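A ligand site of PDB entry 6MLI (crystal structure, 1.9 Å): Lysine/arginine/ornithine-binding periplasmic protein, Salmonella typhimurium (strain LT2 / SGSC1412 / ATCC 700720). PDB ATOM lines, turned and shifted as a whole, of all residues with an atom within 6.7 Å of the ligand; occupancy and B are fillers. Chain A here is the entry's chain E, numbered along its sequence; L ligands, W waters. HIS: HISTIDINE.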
ATOM      1  N   ASP A  11     -13.562  11.558  15.739  1.00  0.00           N
ATOM      2  CA  ASP A  11     -12.232  11.726  15.142  1.00  0.00           C
ATOM      3  C   ASP A  11     -12.407  12.330  13.752  1.00  0.00           C
ATOM      4  O   ASP A  11     -12.864  11.658  12.833  1.00  0.00           O
ATOM      5  CB  ASP A  11     -11.496  10.391  15.089  1.00  0.00           C
ATOM      6  CG  ASP A  11     -10.244  10.421  14.233  1.00  0.00           C
ATOM      7  OD1 ASP A  11      -9.737  11.523  13.917  1.00  0.00           O
ATOM      8  OD2 ASP A  11      -9.758   9.331  13.902  1.00  0.00           O
ATOM      9  N   TYR A  14     -11.739  11.322   9.047  1.00  0.00           N
ATOM     10  CA  TYR A  14     -12.291  10.134   8.394  1.00  0.00           C
ATOM     11  C   TYR A  14     -13.429  10.551   7.436  1.00  0.00           C
ATOM     12  O   TYR A  14     -14.586  10.157   7.613  1.00  0.00           O
ATOM     13  CB  TYR A  14     -12.778   9.142   9.456  1.00  0.00           C
ATOM     14  CG  TYR A  14     -12.427   7.666   9.228  1.00  0.00           C
ATOM     15  CD1 TYR A  14     -11.097   7.244   9.207  1.00  0.00           C
ATOM     16  CD2 TYR A  14     -13.422   6.706   9.088  1.00  0.00           C
ATOM     17  CE1 TYR A  14     -10.766   5.903   9.036  1.00  0.00           C
ATOM     18  CE2 TYR A  14     -13.105   5.367   8.915  1.00  0.00           C
ATOM     19  CZ  TYR A  14     -11.769   4.960   8.877  1.00  0.00           C
ATOM     20  OH  TYR A  14     -11.452   3.621   8.704  1.00  0.00           O
ATOM     21  N   ASP A  30     -21.500  11.183   9.629  1.00  0.00           N
ATOM     22  CA  ASP A  30     -21.594  11.015  11.084  1.00  0.00           C
ATOM     23  C   ASP A  30     -22.173  12.260  11.753  1.00  0.00           C
ATOM     24  O   ASP A  30     -23.014  12.166  12.652  1.00  0.00           O
ATOM     25  CB  ASP A  30     -20.230  10.733  11.723  1.00  0.00           C
ATOM     26  CG  ASP A  30     -19.811   9.274  11.630  1.00  0.00           C
ATOM     27  OD1 ASP A  30     -20.658   8.408  11.284  1.00  0.00           O
ATOM     28  OD2 ASP A  30     -18.642   8.993  11.952  1.00  0.00           O
ATOM     29  N   PHE A  52      -8.854   8.937  17.456  1.00  0.00           N
ATOM     30  CA  PHE A  52      -9.749   7.787  17.592  1.00  0.00           C
ATOM     31  C   PHE A  52      -9.465   6.943  18.837  1.00  0.00           C
ATOM     32  O   PHE A  52     -10.382   6.500  19.526  1.00  0.00           O
ATOM     33  CB  PHE A  52      -9.650   6.918  16.348  1.00  0.00           C
ATOM     34  CG  PHE A  52     -10.656   5.806  16.314  1.00  0.00           C
ATOM     35  CD1 PHE A  52     -11.984   6.076  16.014  1.00  0.00           C
ATOM     36  CD2 PHE A  52     -10.272   4.501  16.567  1.00  0.00           C
ATOM     37  CE1 PHE A  52     -12.918   5.061  15.970  1.00  0.00           C
ATOM     38  CE2 PHE A  52     -11.209   3.476  16.525  1.00  0.00           C
ATOM     39  CZ  PHE A  52     -12.528   3.756  16.231  1.00  0.00           C
ATOM     40  N   SER A  69     -18.270   8.050  15.339  1.00  0.00           N
ATOM     41  CA  SER A  69     -16.972   8.149  14.683  1.00  0.00           C
ATOM     42  C   SER A  69     -16.697   6.880  13.882  1.00  0.00           C
ATOM     43  O   SER A  69     -15.610   6.294  13.995  1.00  0.00           O
ATOM     44  CB  SER A  69     -15.886   8.380  15.742  1.00  0.00           C
ATOM     45  OG  SER A  69     -14.704   8.950  15.182  1.00  0.00           O
ATOM     46  N   SER A  70     -17.686   6.465  13.076  1.00  0.00           N
ATOM     47  CA  SER A  70     -17.615   5.190  12.356  1.00  0.00           C
ATOM     48  C   SER A  70     -17.168   4.054  13.292  1.00  0.00           C
ATOM     49  O   SER A  70     -16.365   3.194  12.908  1.00  0.00           O
ATOM     50  CB  SER A  70     -16.644   5.290  11.168  1.00  0.00           C
ATOM     51  OG  SER A  70     -17.111   6.221  10.195  1.00  0.00           O
ATOM     52  N   LEU A  71     -17.663   4.075  14.525  1.00  0.00           N
ATOM     53  CA  LEU A  71     -17.248   3.090  15.529  1.00  0.00           C
ATOM     54  C   LEU A  71     -17.954   1.749  15.318  1.00  0.00           C
ATOM     55  O   LEU A  71     -19.163   1.637  15.517  1.00  0.00           O
ATOM     56  CB  LEU A  71     -17.521   3.618  16.939  1.00  0.00           C
ATOM     57  CG  LEU A  71     -16.994   2.808  18.122  1.00  0.00           C
ATOM     58  CD1 LEU A  71     -15.455   2.765  18.084  1.00  0.00           C
ATOM     59  CD2 LEU A  71     -17.503   3.388  19.433  1.00  0.00           C
ATOM     60  N   SER A  72     -17.202   0.729  14.919  1.00  0.00           N
ATOM     61  CA  SER A  72     -17.793  -0.586  14.619  1.00  0.00           C
ATOM     62  C   SER A  72     -18.379  -1.319  15.829  1.00  0.00           C
ATOM     63  O   SER A  72     -17.790  -1.337  16.904  1.00  0.00           O
ATOM     64  CB  SER A  72     -16.746  -1.487  13.950  1.00  0.00           C
ATOM     65  OG  SER A  72     -16.458  -1.010  12.656  1.00  0.00           O
ATOM     66  N   ILE A  73     -19.526  -1.954  15.622  1.00  0.00           N
ATOM     67  CA  ILE A  73     -20.186  -2.691  16.699  1.00  0.00           C
ATOM     68  C   ILE A  73     -19.576  -4.085  16.759  1.00  0.00           C
ATOM     69  O   ILE A  73     -19.942  -4.955  15.983  1.00  0.00           O
ATOM     70  CB  ILE A  73     -21.704  -2.769  16.477  1.00  0.00           C
ATOM     71  CG1 ILE A  73     -22.274  -1.365  16.235  1.00  0.00           C
ATOM     72  CG2 ILE A  73     -22.408  -3.446  17.673  1.00  0.00           C
ATOM     73  CD1 ILE A  73     -23.682  -1.361  15.710  1.00  0.00           C
ATOM     74  N   THR A  74     -18.620  -4.282  17.666  1.00  0.00           N
ATOM     75  CA  THR A  74     -17.909  -5.558  17.743  1.00  0.00           C
ATOM     76  C   THR A  74     -18.125  -6.217  19.094  1.00  0.00           C
ATOM     77  O   THR A  74     -18.495  -5.550  20.066  1.00  0.00           O
ATOM     78  CB  THR A  74     -16.411  -5.390  17.533  1.00  0.00           C
ATOM     79  OG1 THR A  74     -15.857  -4.663  18.641  1.00  0.00           O
ATOM     80  CG2 THR A  74     -16.121  -4.653  16.222  1.00  0.00           C
ATOM     81  N   ALA A  90     -20.001  -1.105   7.431  1.00  0.00           N
ATOM     82  CA  ALA A  90     -18.624  -0.698   7.174  1.00  0.00           C
ATOM     83  C   ALA A  90     -17.670  -1.881   6.996  1.00  0.00           C
ATOM     84  O   ALA A  90     -17.276  -2.510   7.968  1.00  0.00           O
ATOM     85  CB  ALA A  90     -18.113   0.202   8.304  1.00  0.00           C
ATOM     86  N   SER A  92     -13.874  -3.446   5.667  1.00  0.00           N
ATOM     87  CA  SER A  92     -12.470  -3.013   5.590  1.00  0.00           C
ATOM     88  C   SER A  92     -11.888  -3.428   4.251  1.00  0.00           C
ATOM     89  O   SER A  92     -12.242  -4.475   3.716  1.00  0.00           O
ATOM     90  CB  SER A  92     -11.645  -3.610   6.721  1.00  0.00           C
ATOM     91  OG  SER A  92     -12.158  -3.281   7.988  1.00  0.00           O
ATOM     92  N   LEU A 117      -4.947   2.681  11.441  1.00  0.00           N
ATOM     93  CA  LEU A 117      -5.311   3.658  12.478  1.00  0.00           C
ATOM     94  C   LEU A 117      -5.166   3.049  13.865  1.00  0.00           C
ATOM     95  O   LEU A 117      -5.718   1.991  14.149  1.00  0.00           O
ATOM     96  CB  LEU A 117      -6.742   4.153  12.268  1.00  0.00           C
ATOM     97  CG  LEU A 117      -7.291   5.149  13.294  1.00  0.00           C
ATOM     98  CD1 LEU A 117      -6.451   6.414  13.319  1.00  0.00           C
ATOM     99  CD2 LEU A 117      -8.743   5.505  13.008  1.00  0.00           C
ATOM    100  N   GLY A 119      -5.764   1.983  17.460  1.00  0.00           N
ATOM    101  CA  GLY A 119      -6.983   1.745  18.228  1.00  0.00           C
ATOM    102  C   GLY A 119      -8.142   1.170  17.423  1.00  0.00           C
ATOM    103  O   GLY A 119      -9.205   0.862  17.963  1.00  0.00           O
ATOM    104  N   SER A 120      -7.962   1.035  16.110  1.00  0.00           N
ATOM    105  CA  SER A 120      -9.022   0.595  15.220  1.00  0.00           C
ATOM    106  C   SER A 120      -9.116  -0.930  15.145  1.00  0.00           C
ATOM    107  O   SER A 120      -8.210  -1.652  15.568  1.00  0.00           O
ATOM    108  CB  SER A 120      -8.824   1.164  13.825  1.00  0.00           C
ATOM    109  OG  SER A 120      -7.688   0.568  13.195  1.00  0.00           O
ATOM    110  N   THR A 121     -10.227  -1.412  14.599  1.00  0.00           N
ATOM    111  CA  THR A 121     -10.378  -2.846  14.323  1.00  0.00           C
ATOM    112  C   THR A 121      -9.369  -3.290  13.277  1.00  0.00           C
ATOM    113  O   THR A 121      -8.917  -4.447  13.292  1.00  0.00           O
ATOM    114  CB  THR A 121     -11.787  -3.178  13.806  1.00  0.00           C
ATOM    115  OG1 THR A 121     -12.043  -2.370  12.655  1.00  0.00           O
ATOM    116  CG2 THR A 121     -12.843  -2.873  14.883  1.00  0.00           C
ATOM    117  N   GLN A 122      -9.021  -2.398  12.366  1.00  0.00           N
ATOM    118  CA  GLN A 122      -7.987  -2.710  11.369  1.00  0.00           C
ATOM    119  C   GLN A 122      -6.624  -2.948  12.017  1.00  0.00           C
ATOM    120  O   GLN A 122      -5.865  -3.835  11.606  1.00  0.00           O
ATOM    121  CB  GLN A 122      -7.861  -1.608  10.324  1.00  0.00           C
ATOM    122  CG  GLN A 122      -9.052  -1.507   9.363  1.00  0.00           C
ATOM    123  CD  GLN A 122     -10.152  -0.630   9.922  1.00  0.00           C
ATOM    124  OE1 GLN A 122      -9.938   0.127  10.872  1.00  0.00           O
ATOM    125  NE2 GLN A 122     -11.344  -0.733   9.340  1.00  0.00           N
ATOM    126  N   GLN A 143      -6.013   9.022  10.458  1.00  0.00           N
ATOM    127  CA  GLN A 143      -6.064   8.504   9.081  1.00  0.00           C
ATOM    128  C   GLN A 143      -5.460   9.457   8.057  1.00  0.00           C
ATOM    129  O   GLN A 143      -4.962   9.034   6.998  1.00  0.00           O
ATOM    130  CB  GLN A 143      -7.523   8.185   8.702  1.00  0.00           C
ATOM    131  CG  GLN A 143      -7.695   7.509   7.338  1.00  0.00           C
ATOM    132  CD  GLN A 143      -7.172   6.083   7.315  1.00  0.00           C
ATOM    133  OE1 GLN A 143      -7.287   5.353   8.291  1.00  0.00           O
ATOM    134  NE2 GLN A 143      -6.578   5.687   6.193  1.00  0.00           N
ATOM    135  N   GLN A 160      -8.264   0.243   6.123  1.00  0.00           N
ATOM    136  CA  GLN A 160      -9.206   1.147   6.774  1.00  0.00           C
ATOM    137  C   GLN A 160     -10.602   0.831   6.247  1.00  0.00           C
ATOM    138  O   GLN A 160     -10.744  -0.109   5.443  1.00  0.00           O
ATOM    139  CB  GLN A 160      -8.844   2.620   6.497  1.00  0.00           C
ATOM    140  CG  GLN A 160      -8.836   3.002   5.019  1.00  0.00           C
ATOM    141  CD  GLN A 160      -7.571   2.547   4.308  1.00  0.00           C
ATOM    142  OE1 GLN A 160      -6.476   2.906   4.722  1.00  0.00           O
ATOM    143  NE2 GLN A 160      -7.719   1.753   3.273  1.00  0.00           N
ATOM    144  N   ASP A 161     -11.616   1.566   6.699  1.00  0.00           N
ATOM    145  CA  ASP A 161     -12.978   1.288   6.232  1.00  0.00           C
ATOM    146  C   ASP A 161     -13.034   1.572   4.721  1.00  0.00           C
ATOM    147  O   ASP A 161     -12.445   2.528   4.225  1.00  0.00           O
ATOM    148  CB  ASP A 161     -14.048   2.096   6.975  1.00  0.00           C
ATOM    149  CG  ASP A 161     -14.318   1.606   8.407  1.00  0.00           C
ATOM    150  OD1 ASP A 161     -13.876   0.501   8.805  1.00  0.00           O
ATOM    151  OD2 ASP A 161     -15.018   2.327   9.150  1.00  0.00           O
ATOM    152  N   PHE A 191     -14.204  -7.188  12.621  1.00  0.00           N
ATOM    153  CA  PHE A 191     -14.713  -5.969  12.016  1.00  0.00           C
ATOM    154  C   PHE A 191     -16.153  -5.632  12.414  1.00  0.00           C
ATOM    155  O   PHE A 191     -16.661  -4.562  12.070  1.00  0.00           O
ATOM    156  CB  PHE A 191     -14.574  -6.068  10.505  1.00  0.00           C
ATOM    157  CG  PHE A 191     -13.146  -6.174  10.051  1.00  0.00           C
ATOM    158  CD1 PHE A 191     -12.201  -5.272  10.509  1.00  0.00           C
ATOM    159  CD2 PHE A 191     -12.728  -7.204   9.240  1.00  0.00           C
ATOM    160  CE1 PHE A 191     -10.856  -5.362  10.130  1.00  0.00           C
ATOM    161  CE2 PHE A 191     -11.392  -7.313   8.857  1.00  0.00           C
ATOM    162  CZ  PHE A 191     -10.465  -6.387   9.314  1.00  0.00           C
ATOM    163  N   GLY A 194     -21.430  -3.282  11.211  1.00  0.00           N
ATOM    164  CA  GLY A 194     -21.808  -1.889  11.024  1.00  0.00           C
ATOM    165  C   GLY A 194     -21.266  -1.048  12.159  1.00  0.00           C
ATOM    166  O   GLY A 194     -20.580  -1.567  13.040  1.00  0.00           O
ATOM    167  N   THR A 195     -21.567   0.255  12.108  1.00  0.00           N
ATOM    168  CA  THR A 195     -21.151   1.215  13.130  1.00  0.00           C
ATOM    169  C   THR A 195     -22.367   1.659  13.931  1.00  0.00           C
ATOM    170  O   THR A 195     -23.491   1.528  13.474  1.00  0.00           O
ATOM    171  CB  THR A 195     -20.472   2.447  12.512  1.00  0.00           C
ATOM    172  OG1 THR A 195     -21.449   3.220  11.788  1.00  0.00           O
ATOM    173  CG2 THR A 195     -19.370   2.035  11.557  1.00  0.00           C
HETATM  174  N   HIS L   1     -14.823   1.216  11.965  1.00  0.00           N
HETATM  175  CA  HIS L   1     -13.506   0.779  12.397  1.00  0.00           C
HETATM  176  C   HIS L   1     -13.372   0.767  13.932  1.00  0.00           C
HETATM  177  O   HIS L   1     -14.383   0.866  14.635  1.00  0.00           O
HETATM  178  CB  HIS L   1     -12.424   1.642  11.732  1.00  0.00           C
HETATM  179  CG  HIS L   1     -12.504   3.103  12.070  1.00  0.00           C
HETATM  180  ND1 HIS L   1     -13.657   3.843  11.923  1.00  0.00           N
HETATM  181  CD2 HIS L   1     -11.541   3.960  12.454  1.00  0.00           C
HETATM  182  CE1 HIS L   1     -13.406   5.102  12.272  1.00  0.00           C
HETATM  183  NE2 HIS L   1     -12.133   5.207  12.591  1.00  0.00           N
HETATM  184  OXT HIS L   1     -12.285   0.633  14.522  1.00  0.00           O
HETATM  185  O   HOH W   1     -15.003  -1.026  17.491  1.00  0.00           O
HETATM  186  O   HOH W   2      -9.575   2.829  10.179  1.00  0.00           O
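N of Ser 70 is in hydrogen-bond range of OD2 of Asp 30, 2.9 Å away. The side-chain hydroxyl (OH) of Tyr 14 lies within hydrogen-bond range of the backbone NH (N) of Asp 161. OE1 of Gln 122 sits at hydrogen-bond distance from OG of Ser 120 (3.3 Å). The side-chain carboxylate of Asp 161 sits at hydrogen-bond distance from the side-chain amide nitrogen of Gln 122 (2.9 Å). The side-chain amide nitrogen (NE2) of Gln 122 sits at hydrogen-bond distance from the side-chain hydroxyl (OG) of Ser 92 (3.0 Å). The side-chain hydroxyl (OG) of Ser 69 is in hydrogen-bond range of the backbone NH (N) of Asp 11. The backbone carbonyl oxygen of Leu 117 sits at hydrogen-bond distance from the side-chain hydroxyl of Ser 120 (2.6 Å).
The side-chain hydroxyl of Ser 72 is in hydrogen-bond range of a nitrogen (N) of the ligand. OD2 of Asp 161 is in salt-bridge range of N of the ligand (3.0 Å). An oxygen (OXT) of the ligand sits at hydrogen-bond distance from the backbone NH of Thr 121 (2.9 Å). The backbone NH (N) of Ser 72 sits at hydrogen-bond distance from an oxygen (O) of the ligand (2.8 Å). The backbone carbonyl oxygen (O) of Ser 70 is in hydrogen-bond range of a nitrogen (N) of the ligand, 2.7 Å away.
Merely in contact with the ligand: Tyr 14 (3.4 Å), Phe 52 (3.5 Å), Ser 69 (3.0 Å), Leu 71 (3.7 Å), Leu 117 (3.2 Å), Ser 120 (3.3 Å) and Gln 122 (3.0 Å). Hydrophobic or aromatic side chains within 4 Å of the ligand: Tyr 14, Phe 52 and Leu 117. Along chain A the residues within 4 Å of the ligand span positions 14 to 161.
Water W2 lies within hydrogen-bond range of OH of Tyr 14 (2.5 Å) and OE1 of Gln 122 (2.8 Å). Water W1 lies within hydrogen-bond range of O of Ser 72 (2.9 Å) and O of the ligand (3.5 Å).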
